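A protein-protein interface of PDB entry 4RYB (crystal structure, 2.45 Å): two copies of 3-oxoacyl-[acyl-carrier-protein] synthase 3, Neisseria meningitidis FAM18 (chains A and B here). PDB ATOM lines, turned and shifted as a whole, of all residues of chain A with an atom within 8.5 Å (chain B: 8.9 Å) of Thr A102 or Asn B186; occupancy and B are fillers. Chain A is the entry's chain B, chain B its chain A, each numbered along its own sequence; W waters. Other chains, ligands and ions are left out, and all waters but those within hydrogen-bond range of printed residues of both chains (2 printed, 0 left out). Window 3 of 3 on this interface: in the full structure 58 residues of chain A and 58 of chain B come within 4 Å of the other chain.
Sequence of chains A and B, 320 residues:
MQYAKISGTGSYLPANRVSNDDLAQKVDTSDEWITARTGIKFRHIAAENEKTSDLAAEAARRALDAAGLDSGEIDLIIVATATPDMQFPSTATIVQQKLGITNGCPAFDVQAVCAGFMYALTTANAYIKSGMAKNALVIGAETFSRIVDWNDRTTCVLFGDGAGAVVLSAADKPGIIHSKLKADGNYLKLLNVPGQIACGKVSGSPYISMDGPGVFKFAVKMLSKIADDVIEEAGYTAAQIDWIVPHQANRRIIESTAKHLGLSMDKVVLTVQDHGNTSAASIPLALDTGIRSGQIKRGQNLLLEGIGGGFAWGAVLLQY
The backbone NH (N) of Asp B184 lies close to the side-chain amide oxygen (OE1) of Gln A96 (3.4 Å). NZ of Lys B182 is in hydrogen-bond range of O of Gly A104. The side-chain amide nitrogen (NE2) of Gln A96 sits at hydrogen-bond distance from the backbone carbonyl oxygen (O) of Ala B183 (3.0 Å). The backbone NH (N) of Ala B183 lies within hydrogen-bond range of the backbone carbonyl oxygen (O) of Gly A104, at 3.2 Å. The backbone NH (N) of Ala B183 sits at hydrogen-bond distance from the backbone carbonyl oxygen (O) of Cys A105 (3.3 Å). OD1 of Asn B186 lies within hydrogen-bond range of NE2 of Gln A97 (3.2 Å). N of Gly B185 is in hydrogen-bond range of OE1 of Gln A96.
The backbone NH (N) of Cys A105 sits at hydrogen-bond distance from the side-chain amide oxygen (OD1) of Asn A103, 3.0 Å away. The backbone carbonyl oxygen (O) of Ile A74 sits at hydrogen-bond distance from the side-chain amide nitrogen (ND2) of Asn A103 (2.9 Å). O of Gln A96 lies within hydrogen-bond range of N of Ile A101 (3.1 Å). N of Asp B184 is in hydrogen-bond range of O of Phe B311 (2.8 Å). The side-chain amide nitrogen of Asn A103 lies within hydrogen-bond range of the backbone carbonyl oxygen of Gly A72 (2.8 Å). The side-chain amide nitrogen (NE2) of Gln A96 is in hydrogen-bond range of the backbone carbonyl oxygen (O) of Cys A105, at 2.8 Å.
Among the printed residues, pairs that only touch across the chains: Thr A93 with Gly B185 (3.4 Å), Gln A97 with Gly B185 (3.4 Å), Thr A102 with Asn B186 (3.8 Å) and Asn A103 with Lys B182 (3.8 Å).
Thr A102 touches just one residue of chain B: Asn B186 (3.8 Å). Asn B186 touches two residues of chain A. Gly B185 touches just these residues of chain A: Thr A93 (3.4 Å), Gln A96 (3.1 Å) and Gln A97 (3.4 Å). Printed residues of chain B within 4 Å of Gly A104: Lys B182 and Ala B183. Of the printed residues of chain A, Asp B184 touches Gln A96 (3.3 Å). Of the printed residues of chain B, Gln A97 touches Gly B185 (3.4 Å) and Asn B186 (3.2 Å). The nearest printed residue of chain B that does not touch Asn A103 is Ala B183 (5.4 Å).
Of the 16 printed residues of chain B, 5 touch a printed residue of chain A. Hydrophobic or aromatic side chains of chain B within 4 Å of the printed part of chain A: Ala B183. Printed residues of chain A that touch a printed residue of chain B: Thr A93, Gln A96, Gln A97, Thr A102, Asn A103, Gly A104 and Cys A105. Among the printed residues, 11 pairs touch across the chains. Among the printed residues, no Asp or Glu carboxylate lies within 4 Å of a Lys or Arg side-chain nitrogen of the other chain.
No position is printed for both chains. Of the 11 pairs that touch across the chains among the printed residues, none has its exchanged pair printed and touching as well.
Water W1 lies within hydrogen-bond range of OG1 of Thr A93 (2.7 Å) and O of Gly B310 (2.8 Å). Water W2 lies within hydrogen-bond range of O of Ala B183, N of Gly A104, O of Ile A101 and NE2 of Gln A96.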
ATOM      1  N   SER A  71     -22.883  20.748  15.058  1.00  0.00           N
ATOM      2  CA  SER A  71     -22.190  20.806  16.340  1.00  0.00           C
ATOM      3  C   SER A  71     -22.907  19.945  17.377  1.00  0.00           C
ATOM      4  O   SER A  71     -22.271  19.317  18.225  1.00  0.00           O
ATOM      5  CB  SER A  71     -22.087  22.254  16.828  1.00  0.00           C
ATOM      6  OG  SER A  71     -23.361  22.777  17.158  1.00  0.00           O
ATOM      7  N   GLY A  72     -24.232  19.910  17.288  1.00  0.00           N
ATOM      8  CA  GLY A  72     -25.053  19.165  18.225  1.00  0.00           C
ATOM      9  C   GLY A  72     -24.881  17.659  18.133  1.00  0.00           C
ATOM     10  O   GLY A  72     -25.373  16.925  18.991  1.00  0.00           O
ATOM     11  N   GLU A  73     -24.200  17.197  17.087  1.00  0.00           N
ATOM     12  CA  GLU A  73     -23.940  15.771  16.899  1.00  0.00           C
ATOM     13  C   GLU A  73     -22.732  15.298  17.709  1.00  0.00           C
ATOM     14  O   GLU A  73     -22.525  14.097  17.879  1.00  0.00           O
ATOM     15  CB  GLU A  73     -23.710  15.460  15.418  1.00  0.00           C
ATOM     16  CG  GLU A  73     -24.972  15.396  14.577  1.00  0.00           C
ATOM     17  CD  GLU A  73     -25.867  14.234  14.957  1.00  0.00           C
ATOM     18  OE1 GLU A  73     -26.885  14.464  15.642  1.00  0.00           O
ATOM     19  OE2 GLU A  73     -25.553  13.091  14.564  1.00  0.00           O
ATOM     20  N   ILE A  74     -21.940  16.243  18.206  1.00  0.00           N
ATOM     21  CA  ILE A  74     -20.739  15.909  18.965  1.00  0.00           C
ATOM     22  C   ILE A  74     -21.086  15.467  20.384  1.00  0.00           C
ATOM     23  O   ILE A  74     -21.789  16.171  21.110  1.00  0.00           O
ATOM     24  CB  ILE A  74     -19.768  17.110  19.020  1.00  0.00           C
ATOM     25  CG1 ILE A  74     -19.304  17.490  17.610  1.00  0.00           C
ATOM     26  CG2 ILE A  74     -18.574  16.815  19.932  1.00  0.00           C
ATOM     27  CD1 ILE A  74     -18.470  16.422  16.911  1.00  0.00           C
ATOM     28  N   ILE A  77     -15.633  16.042  23.402  1.00  0.00           N
ATOM     29  CA  ILE A  77     -14.676  17.077  23.027  1.00  0.00           C
ATOM     30  C   ILE A  77     -13.418  16.941  23.876  1.00  0.00           C
ATOM     31  O   ILE A  77     -13.485  16.981  25.101  1.00  0.00           O
ATOM     32  CB  ILE A  77     -15.270  18.487  23.202  1.00  0.00           C
ATOM     33  CG1 ILE A  77     -16.557  18.620  22.379  1.00  0.00           C
ATOM     34  CG2 ILE A  77     -14.244  19.550  22.806  1.00  0.00           C
ATOM     35  CD1 ILE A  77     -17.301  19.924  22.585  1.00  0.00           C
ATOM     36  N   THR A  93     -14.214  23.165  27.565  1.00  0.00           N
ATOM     37  CA  THR A  93     -15.552  23.664  27.890  1.00  0.00           C
ATOM     38  C   THR A  93     -15.765  25.048  27.286  1.00  0.00           C
ATOM     39  O   THR A  93     -16.865  25.375  26.843  1.00  0.00           O
ATOM     40  CB  THR A  93     -15.799  23.741  29.416  1.00  0.00           C
ATOM     41  OG1 THR A  93     -14.791  24.550  30.035  1.00  0.00           O
ATOM     42  CG2 THR A  93     -15.800  22.351  30.037  1.00  0.00           C
ATOM     43  N   ILE A  94     -14.711  25.856  27.275  1.00  0.00           N
ATOM     44  CA  ILE A  94     -14.772  27.179  26.667  1.00  0.00           C
ATOM     45  C   ILE A  94     -15.007  27.034  25.167  1.00  0.00           C
ATOM     46  O   ILE A  94     -15.827  27.750  24.589  1.00  0.00           O
ATOM     47  CB  ILE A  94     -13.481  27.988  26.929  1.00  0.00           C
ATOM     48  CG1 ILE A  94     -13.319  28.245  28.429  1.00  0.00           C
ATOM     49  CG2 ILE A  94     -13.498  29.311  26.165  1.00  0.00           C
ATOM     50  CD1 ILE A  94     -11.966  28.803  28.827  1.00  0.00           C
ATOM     51  N   GLN A  96     -16.353  24.406  23.757  1.00  0.00           N
ATOM     52  CA  GLN A  96     -17.705  23.866  23.671  1.00  0.00           C
ATOM     53  C   GLN A  96     -18.720  24.995  23.644  1.00  0.00           C
ATOM     54  O   GLN A  96     -19.642  25.005  22.828  1.00  0.00           O
ATOM     55  CB  GLN A  96     -17.983  22.934  24.848  1.00  0.00           C
ATOM     56  CG  GLN A  96     -19.330  22.227  24.788  1.00  0.00           C
ATOM     57  CD  GLN A  96     -19.701  21.586  26.112  1.00  0.00           C
ATOM     58  OE1 GLN A  96     -19.611  22.215  27.165  1.00  0.00           O
ATOM     59  NE2 GLN A  96     -20.124  20.327  26.063  1.00  0.00           N
ATOM     60  N   GLN A  97     -18.534  25.951  24.547  1.00  0.00           N
ATOM     61  CA  GLN A  97     -19.423  27.098  24.658  1.00  0.00           C
ATOM     62  C   GLN A  97     -19.382  27.938  23.386  1.00  0.00           C
ATOM     63  O   GLN A  97     -20.420  28.359  22.877  1.00  0.00           O
ATOM     64  CB  GLN A  97     -19.037  27.943  25.877  1.00  0.00           C
ATOM     65  CG  GLN A  97     -20.082  28.957  26.312  1.00  0.00           C
ATOM     66  CD  GLN A  97     -20.135  30.176  25.415  1.00  0.00           C
ATOM     67  OE1 GLN A  97     -19.104  30.700  24.995  1.00  0.00           O
ATOM     68  NE2 GLN A  97     -21.344  30.636  25.114  1.00  0.00           N
ATOM     69  N   LYS A  98     -18.180  28.160  22.868  1.00  0.00           N
ATOM     70  CA  LYS A  98     -17.997  29.004  21.694  1.00  0.00           C
ATOM     71  C   LYS A  98     -18.525  28.337  20.427  1.00  0.00           C
ATOM     72  O   LYS A  98     -18.879  29.018  19.466  1.00  0.00           O
ATOM     73  CB  LYS A  98     -16.520  29.366  21.530  1.00  0.00           C
ATOM     74  CG  LYS A  98     -16.064  30.432  22.510  1.00  0.00           C
ATOM     75  CD  LYS A  98     -14.599  30.794  22.345  1.00  0.00           C
ATOM     76  CE  LYS A  98     -14.159  31.746  23.447  1.00  0.00           C
ATOM     77  NZ  LYS A  98     -12.801  32.305  23.219  1.00  0.00           N
ATOM     78  N   LEU A  99     -18.569  27.008  20.422  1.00  0.00           N
ATOM     79  CA  LEU A  99     -19.148  26.275  19.302  1.00  0.00           C
ATOM     80  C   LEU A  99     -20.675  26.220  19.402  1.00  0.00           C
ATOM     81  O   LEU A  99     -21.352  25.770  18.476  1.00  0.00           O
ATOM     82  CB  LEU A  99     -18.579  24.855  19.241  1.00  0.00           C
ATOM     83  CG  LEU A  99     -17.098  24.723  18.872  1.00  0.00           C
ATOM     84  CD1 LEU A  99     -16.652  23.280  19.031  1.00  0.00           C
ATOM     85  CD2 LEU A  99     -16.829  25.208  17.459  1.00  0.00           C
ATOM     86  N   GLY A 100     -21.215  26.691  20.522  1.00  0.00           N
ATOM     87  CA  GLY A 100     -22.651  26.677  20.740  1.00  0.00           C
ATOM     88  C   GLY A 100     -23.218  25.289  20.980  1.00  0.00           C
ATOM     89  O   GLY A 100     -24.390  25.038  20.707  1.00  0.00           O
ATOM     90  N   ILE A 101     -22.389  24.388  21.498  1.00  0.00           N
ATOM     91  CA  ILE A 101     -22.834  23.037  21.821  1.00  0.00           C
ATOM     92  C   ILE A 101     -23.429  23.014  23.222  1.00  0.00           C
ATOM     93  O   ILE A 101     -22.717  23.184  24.209  1.00  0.00           O
ATOM     94  CB  ILE A 101     -21.682  22.018  21.723  1.00  0.00           C
ATOM     95  CG1 ILE A 101     -21.180  21.943  20.278  1.00  0.00           C
ATOM     96  CG2 ILE A 101     -22.142  20.643  22.212  1.00  0.00           C
ATOM     97  CD1 ILE A 101     -20.004  21.005  20.058  1.00  0.00           C
ATOM     98  N   THR A 102     -24.737  22.789  23.297  1.00  0.00           N
ATOM     99  CA  THR A 102     -25.450  22.786  24.570  1.00  0.00           C
ATOM    100  C   THR A 102     -26.113  21.441  24.845  1.00  0.00           C
ATOM    101  O   THR A 102     -27.011  21.347  25.681  1.00  0.00           O
ATOM    102  CB  THR A 102     -26.529  23.881  24.598  1.00  0.00           C
ATOM    103  OG1 THR A 102     -27.488  23.637  23.560  1.00  0.00           O
ATOM    104  CG2 THR A 102     -25.903  25.252  24.394  1.00  0.00           C
ATOM    105  N   ASN A 103     -25.672  20.404  24.137  1.00  0.00           N
ATOM    106  CA  ASN A 103     -26.213  19.064  24.340  1.00  0.00           C
ATOM    107  C   ASN A 103     -25.612  18.378  25.572  1.00  0.00           C
ATOM    108  O   ASN A 103     -25.939  17.229  25.875  1.00  0.00           O
ATOM    109  CB  ASN A 103     -25.993  18.208  23.088  1.00  0.00           C
ATOM    110  CG  ASN A 103     -24.529  18.066  22.711  1.00  0.00           C
ATOM    111  OD1 ASN A 103     -23.632  18.343  23.507  1.00  0.00           O
ATOM    112  ND2 ASN A 103     -24.283  17.633  21.479  1.00  0.00           N
ATOM    113  N   GLY A 104     -24.736  19.087  26.277  1.00  0.00           N
ATOM    114  CA  GLY A 104     -24.160  18.584  27.511  1.00  0.00           C
ATOM    115  C   GLY A 104     -23.077  17.532  27.342  1.00  0.00           C
ATOM    116  O   GLY A 104     -22.817  16.772  28.272  1.00  0.00           O
ATOM    117  N   CYS A 105     -22.440  17.481  26.176  1.00  0.00           N
ATOM    118  CA  CYS A 105     -21.429  16.454  25.922  1.00  0.00           C
ATOM    119  C   CYS A 105     -20.200  16.668  26.801  1.00  0.00           C
ATOM    120  O   CYS A 105     -19.891  17.801  27.167  1.00  0.00           O
ATOM    121  CB  CYS A 105     -21.012  16.429  24.448  1.00  0.00           C
ATOM    122  SG  CYS A 105     -19.881  17.746  23.937  1.00  0.00           S
ATOM    123  N   LYS B 182     -20.686  14.802  31.615  1.00  0.00           N
ATOM    124  CA  LYS B 182     -21.358  15.945  31.006  1.00  0.00           C
ATOM    125  C   LYS B 182     -20.555  17.225  31.177  1.00  0.00           C
ATOM    126  O   LYS B 182     -19.692  17.319  32.051  1.00  0.00           O
ATOM    127  CB  LYS B 182     -22.760  16.137  31.591  1.00  0.00           C
ATOM    128  CG  LYS B 182     -23.805  15.157  31.076  1.00  0.00           C
ATOM    129  CD  LYS B 182     -25.051  15.911  30.592  1.00  0.00           C
ATOM    130  CE  LYS B 182     -25.823  15.192  29.483  1.00  0.00           C
ATOM    131  NZ  LYS B 182     -24.959  14.558  28.442  1.00  0.00           N
ATOM    132  N   ALA B 183     -20.837  18.202  30.322  1.00  0.00           N
ATOM    133  CA  ALA B 183     -20.199  19.507  30.419  1.00  0.00           C
ATOM    134  C   ALA B 183     -21.015  20.557  29.680  1.00  0.00           C
ATOM    135  O   ALA B 183     -21.630  20.270  28.657  1.00  0.00           O
ATOM    136  CB  ALA B 183     -18.782  19.452  29.870  1.00  0.00           C
ATOM    137  N   ASP B 184     -21.000  21.776  30.204  1.00  0.00           N
ATOM    138  CA  ASP B 184     -21.695  22.895  29.584  1.00  0.00           C
ATOM    139  C   ASP B 184     -20.941  24.180  29.898  1.00  0.00           C
ATOM    140  O   ASP B 184     -20.968  24.671  31.027  1.00  0.00           O
ATOM    141  CB  ASP B 184     -23.142  22.980  30.078  1.00  0.00           C
ATOM    142  CG  ASP B 184     -24.018  23.831  29.175  1.00  0.00           C
ATOM    143  OD1 ASP B 184     -23.497  24.786  28.560  1.00  0.00           O
ATOM    144  OD2 ASP B 184     -25.232  23.546  29.082  1.00  0.00           O
ATOM    145  N   GLY B 185     -20.260  24.711  28.889  1.00  0.00           N
ATOM    146  CA  GLY B 185     -19.399  25.867  29.057  1.00  0.00           C
ATOM    147  C   GLY B 185     -20.126  27.171  29.322  1.00  0.00           C
ATOM    148  O   GLY B 185     -19.490  28.203  29.528  1.00  0.00           O
ATOM    149  N   ASN B 186     -21.455  27.133  29.314  1.00  0.00           N
ATOM    150  CA  ASN B 186     -22.252  28.324  29.597  1.00  0.00           C
ATOM    151  C   ASN B 186     -22.170  28.756  31.057  1.00  0.00           C
ATOM    152  O   ASN B 186     -22.554  29.875  31.398  1.00  0.00           O
ATOM    153  CB  ASN B 186     -23.717  28.085  29.229  1.00  0.00           C
ATOM    154  CG  ASN B 186     -24.015  28.392  27.777  1.00  0.00           C
ATOM    155  OD1 ASN B 186     -23.464  29.332  27.203  1.00  0.00           O
ATOM    156  ND2 ASN B 186     -24.890  27.598  27.173  1.00  0.00           N
ATOM    157  N   TYR B 187     -21.674  27.865  31.913  1.00  0.00           N
ATOM    158  CA  TYR B 187     -21.598  28.126  33.348  1.00  0.00           C
ATOM    159  C   TYR B 187     -20.179  28.481  33.792  1.00  0.00           C
ATOM    160  O   TYR B 187     -19.808  28.261  34.945  1.00  0.00           O
ATOM    161  CB  TYR B 187     -22.102  26.910  34.127  1.00  0.00           C
ATOM    162  CG  TYR B 187     -23.546  26.573  33.843  1.00  0.00           C
ATOM    163  CD1 TYR B 187     -24.573  27.265  34.467  1.00  0.00           C
ATOM    164  CD2 TYR B 187     -23.883  25.567  32.947  1.00  0.00           C
ATOM    165  CE1 TYR B 187     -25.893  26.965  34.212  1.00  0.00           C
ATOM    166  CE2 TYR B 187     -25.203  25.260  32.685  1.00  0.00           C
ATOM    167  CZ  TYR B 187     -26.205  25.963  33.320  1.00  0.00           C
ATOM    168  OH  TYR B 187     -27.523  25.665  33.068  1.00  0.00           O
ATOM    169  N   LEU B 188     -19.394  29.034  32.874  1.00  0.00           N
ATOM    170  CA  LEU B 188     -18.021  29.430  33.170  1.00  0.00           C
ATOM    171  C   LEU B 188     -17.952  30.457  34.299  1.00  0.00           C
ATOM    172  O   LEU B 188     -17.159  30.323  35.231  1.00  0.00           O
ATOM    173  CB  LEU B 188     -17.364  30.002  31.910  1.00  0.00           C
ATOM    174  CG  LEU B 188     -16.075  30.813  32.061  1.00  0.00           C
ATOM    175  CD1 LEU B 188     -14.887  29.894  32.271  1.00  0.00           C
ATOM    176  CD2 LEU B 188     -15.872  31.705  30.846  1.00  0.00           C
ATOM    177  N   LYS B 189     -18.783  31.454  34.184  1.00  0.00           N
ATOM    178  CA  LYS B 189     -18.783  32.564  35.081  1.00  0.00           C
ATOM    179  C   LYS B 189     -19.083  32.262  36.517  1.00  0.00           C
ATOM    180  O   LYS B 189     -18.825  33.089  37.329  1.00  0.00           O
ATOM    181  CB  LYS B 189     -19.705  33.668  34.564  1.00  0.00           C
ATOM    182  CG  LYS B 189     -19.117  34.411  33.398  1.00  0.00           C
ATOM    183  CD  LYS B 189     -20.131  35.034  32.461  1.00  0.00           C
ATOM    184  CE  LYS B 189     -21.324  34.129  32.150  1.00  0.00           C
ATOM    185  NZ  LYS B 189     -21.954  34.456  30.830  1.00  0.00           N
ATOM    186  N   LEU B 190     -19.608  31.085  36.804  1.00  0.00           N
ATOM    187  CA  LEU B 190     -20.052  30.699  38.145  1.00  0.00           C
ATOM    188  C   LEU B 190     -18.909  30.161  39.005  1.00  0.00           C
ATOM    189  O   LEU B 190     -18.978  30.209  40.233  1.00  0.00           O
ATOM    190  CB  LEU B 190     -21.171  29.658  38.056  1.00  0.00           C
ATOM    191  CG  LEU B 190     -22.582  30.209  37.829  1.00  0.00           C
ATOM    192  CD1 LEU B 190     -22.652  31.103  36.599  1.00  0.00           C
ATOM    193  CD2 LEU B 190     -23.578  29.066  37.713  1.00  0.00           C
ATOM    194  N   LEU B 191     -17.865  29.642  38.367  1.00  0.00           N
ATOM    195  CA  LEU B 191     -16.699  29.145  39.093  1.00  0.00           C
ATOM    196  C   LEU B 191     -15.495  29.078  38.163  1.00  0.00           C
ATOM    197  O   LEU B 191     -15.487  28.314  37.197  1.00  0.00           O
ATOM    198  CB  LEU B 191     -16.976  27.769  39.701  1.00  0.00           C
ATOM    199  CG  LEU B 191     -15.826  27.135  40.494  1.00  0.00           C
ATOM    200  CD1 LEU B 191     -15.308  28.079  41.572  1.00  0.00           C
ATOM    201  CD2 LEU B 191     -16.264  25.823  41.117  1.00  0.00           C
ATOM    202  N   PHE B 218     -27.578  25.072  40.650  1.00  0.00           N
ATOM    203  CA  PHE B 218     -27.447  24.166  39.514  1.00  0.00           C
ATOM    204  C   PHE B 218     -26.898  22.798  39.911  1.00  0.00           C
ATOM    205  O   PHE B 218     -27.240  21.789  39.295  1.00  0.00           O
ATOM    206  CB  PHE B 218     -26.565  24.807  38.440  1.00  0.00           C
ATOM    207  CG  PHE B 218     -27.218  25.971  37.745  1.00  0.00           C
ATOM    208  CD1 PHE B 218     -28.272  25.769  36.867  1.00  0.00           C
ATOM    209  CD2 PHE B 218     -26.787  27.267  37.975  1.00  0.00           C
ATOM    210  CE1 PHE B 218     -28.879  26.835  36.230  1.00  0.00           C
ATOM    211  CE2 PHE B 218     -27.389  28.338  37.340  1.00  0.00           C
ATOM    212  CZ  PHE B 218     -28.437  28.121  36.468  1.00  0.00           C
ATOM    213  N   MET B 222     -28.526  19.496  38.649  1.00  0.00           N
ATOM    214  CA  MET B 222     -27.784  18.643  37.727  1.00  0.00           C
ATOM    215  C   MET B 222     -27.453  17.273  38.313  1.00  0.00           C
ATOM    216  O   MET B 222     -27.577  16.254  37.634  1.00  0.00           O
ATOM    217  CB  MET B 222     -26.490  19.344  37.302  1.00  0.00           C
ATOM    218  CG  MET B 222     -26.704  20.524  36.361  1.00  0.00           C
ATOM    219  SD  MET B 222     -25.209  21.503  36.091  1.00  0.00           S
ATOM    220  CE  MET B 222     -25.865  22.876  35.146  1.00  0.00           C
ATOM    221  N   GLY B 310     -16.734  24.686  34.989  1.00  0.00           N
ATOM    222  CA  GLY B 310     -16.899  24.394  33.577  1.00  0.00           C
ATOM    223  C   GLY B 310     -18.185  24.981  33.019  1.00  0.00           C
ATOM    224  O   GLY B 310     -18.133  25.896  32.201  1.00  0.00           O
ATOM    225  N   PHE B 311     -19.340  24.468  33.445  1.00  0.00           N
ATOM    226  CA  PHE B 311     -19.428  23.339  34.370  1.00  0.00           C
ATOM    227  C   PHE B 311     -19.078  22.019  33.698  1.00  0.00           C
ATOM    228  O   PHE B 311     -19.373  21.802  32.524  1.00  0.00           O
ATOM    229  CB  PHE B 311     -20.837  23.229  34.969  1.00  0.00           C
ATOM    230  CG  PHE B 311     -21.153  24.268  36.018  1.00  0.00           C
ATOM    231  CD1 PHE B 311     -20.150  24.982  36.658  1.00  0.00           C
ATOM    232  CD2 PHE B 311     -22.468  24.515  36.373  1.00  0.00           C
ATOM    233  CE1 PHE B 311     -20.457  25.927  37.619  1.00  0.00           C
ATOM    234  CE2 PHE B 311     -22.778  25.456  37.332  1.00  0.00           C
ATOM    235  CZ  PHE B 311     -21.774  26.163  37.955  1.00  0.00           C
ATOM    236  N   ALA B 312     -18.440  21.148  34.470  1.00  0.00           N
ATOM    237  CA  ALA B 312     -18.273  19.750  34.104  1.00  0.00           C
ATOM    238  C   ALA B 312     -18.757  18.905  35.271  1.00  0.00           C
ATOM    239  O   ALA B 312     -18.472  19.214  36.426  1.00  0.00           O
ATOM    240  CB  ALA B 312     -16.819  19.442  33.774  1.00  0.00           C
ATOM    241  N   TRP B 313     -19.502  17.851  34.969  1.00  0.00           N
ATOM    242  CA  TRP B 313     -20.010  16.973  36.008  1.00  0.00           C
ATOM    243  C   TRP B 313     -20.196  15.566  35.471  1.00  0.00           C
ATOM    244  O   TRP B 313     -20.142  15.334  34.263  1.00  0.00           O
ATOM    245  CB  TRP B 313     -21.326  17.511  36.585  1.00  0.00           C
ATOM    246  CG  TRP B 313     -22.504  17.501  35.654  1.00  0.00           C
ATOM    247  CD1 TRP B 313     -23.530  16.603  35.647  1.00  0.00           C
ATOM    248  CD2 TRP B 313     -22.791  18.445  34.612  1.00  0.00           C
ATOM    249  NE1 TRP B 313     -24.434  16.921  34.664  1.00  0.00           N
ATOM    250  CE2 TRP B 313     -24.005  18.047  34.014  1.00  0.00           C
ATOM    251  CE3 TRP B 313     -22.140  19.581  34.126  1.00  0.00           C
ATOM    252  CZ2 TRP B 313     -24.578  18.746  32.953  1.00  0.00           C
ATOM    253  CZ3 TRP B 313     -22.712  20.273  33.070  1.00  0.00           C
ATOM    254  CH2 TRP B 313     -23.917  19.852  32.496  1.00  0.00           C
HETATM  255  O   HOH W   1     -16.132  26.794  30.519  1.00  0.00           O
HETATM  256  O   HOH W   2     -23.315  21.484  26.747  1.00  0.00           O
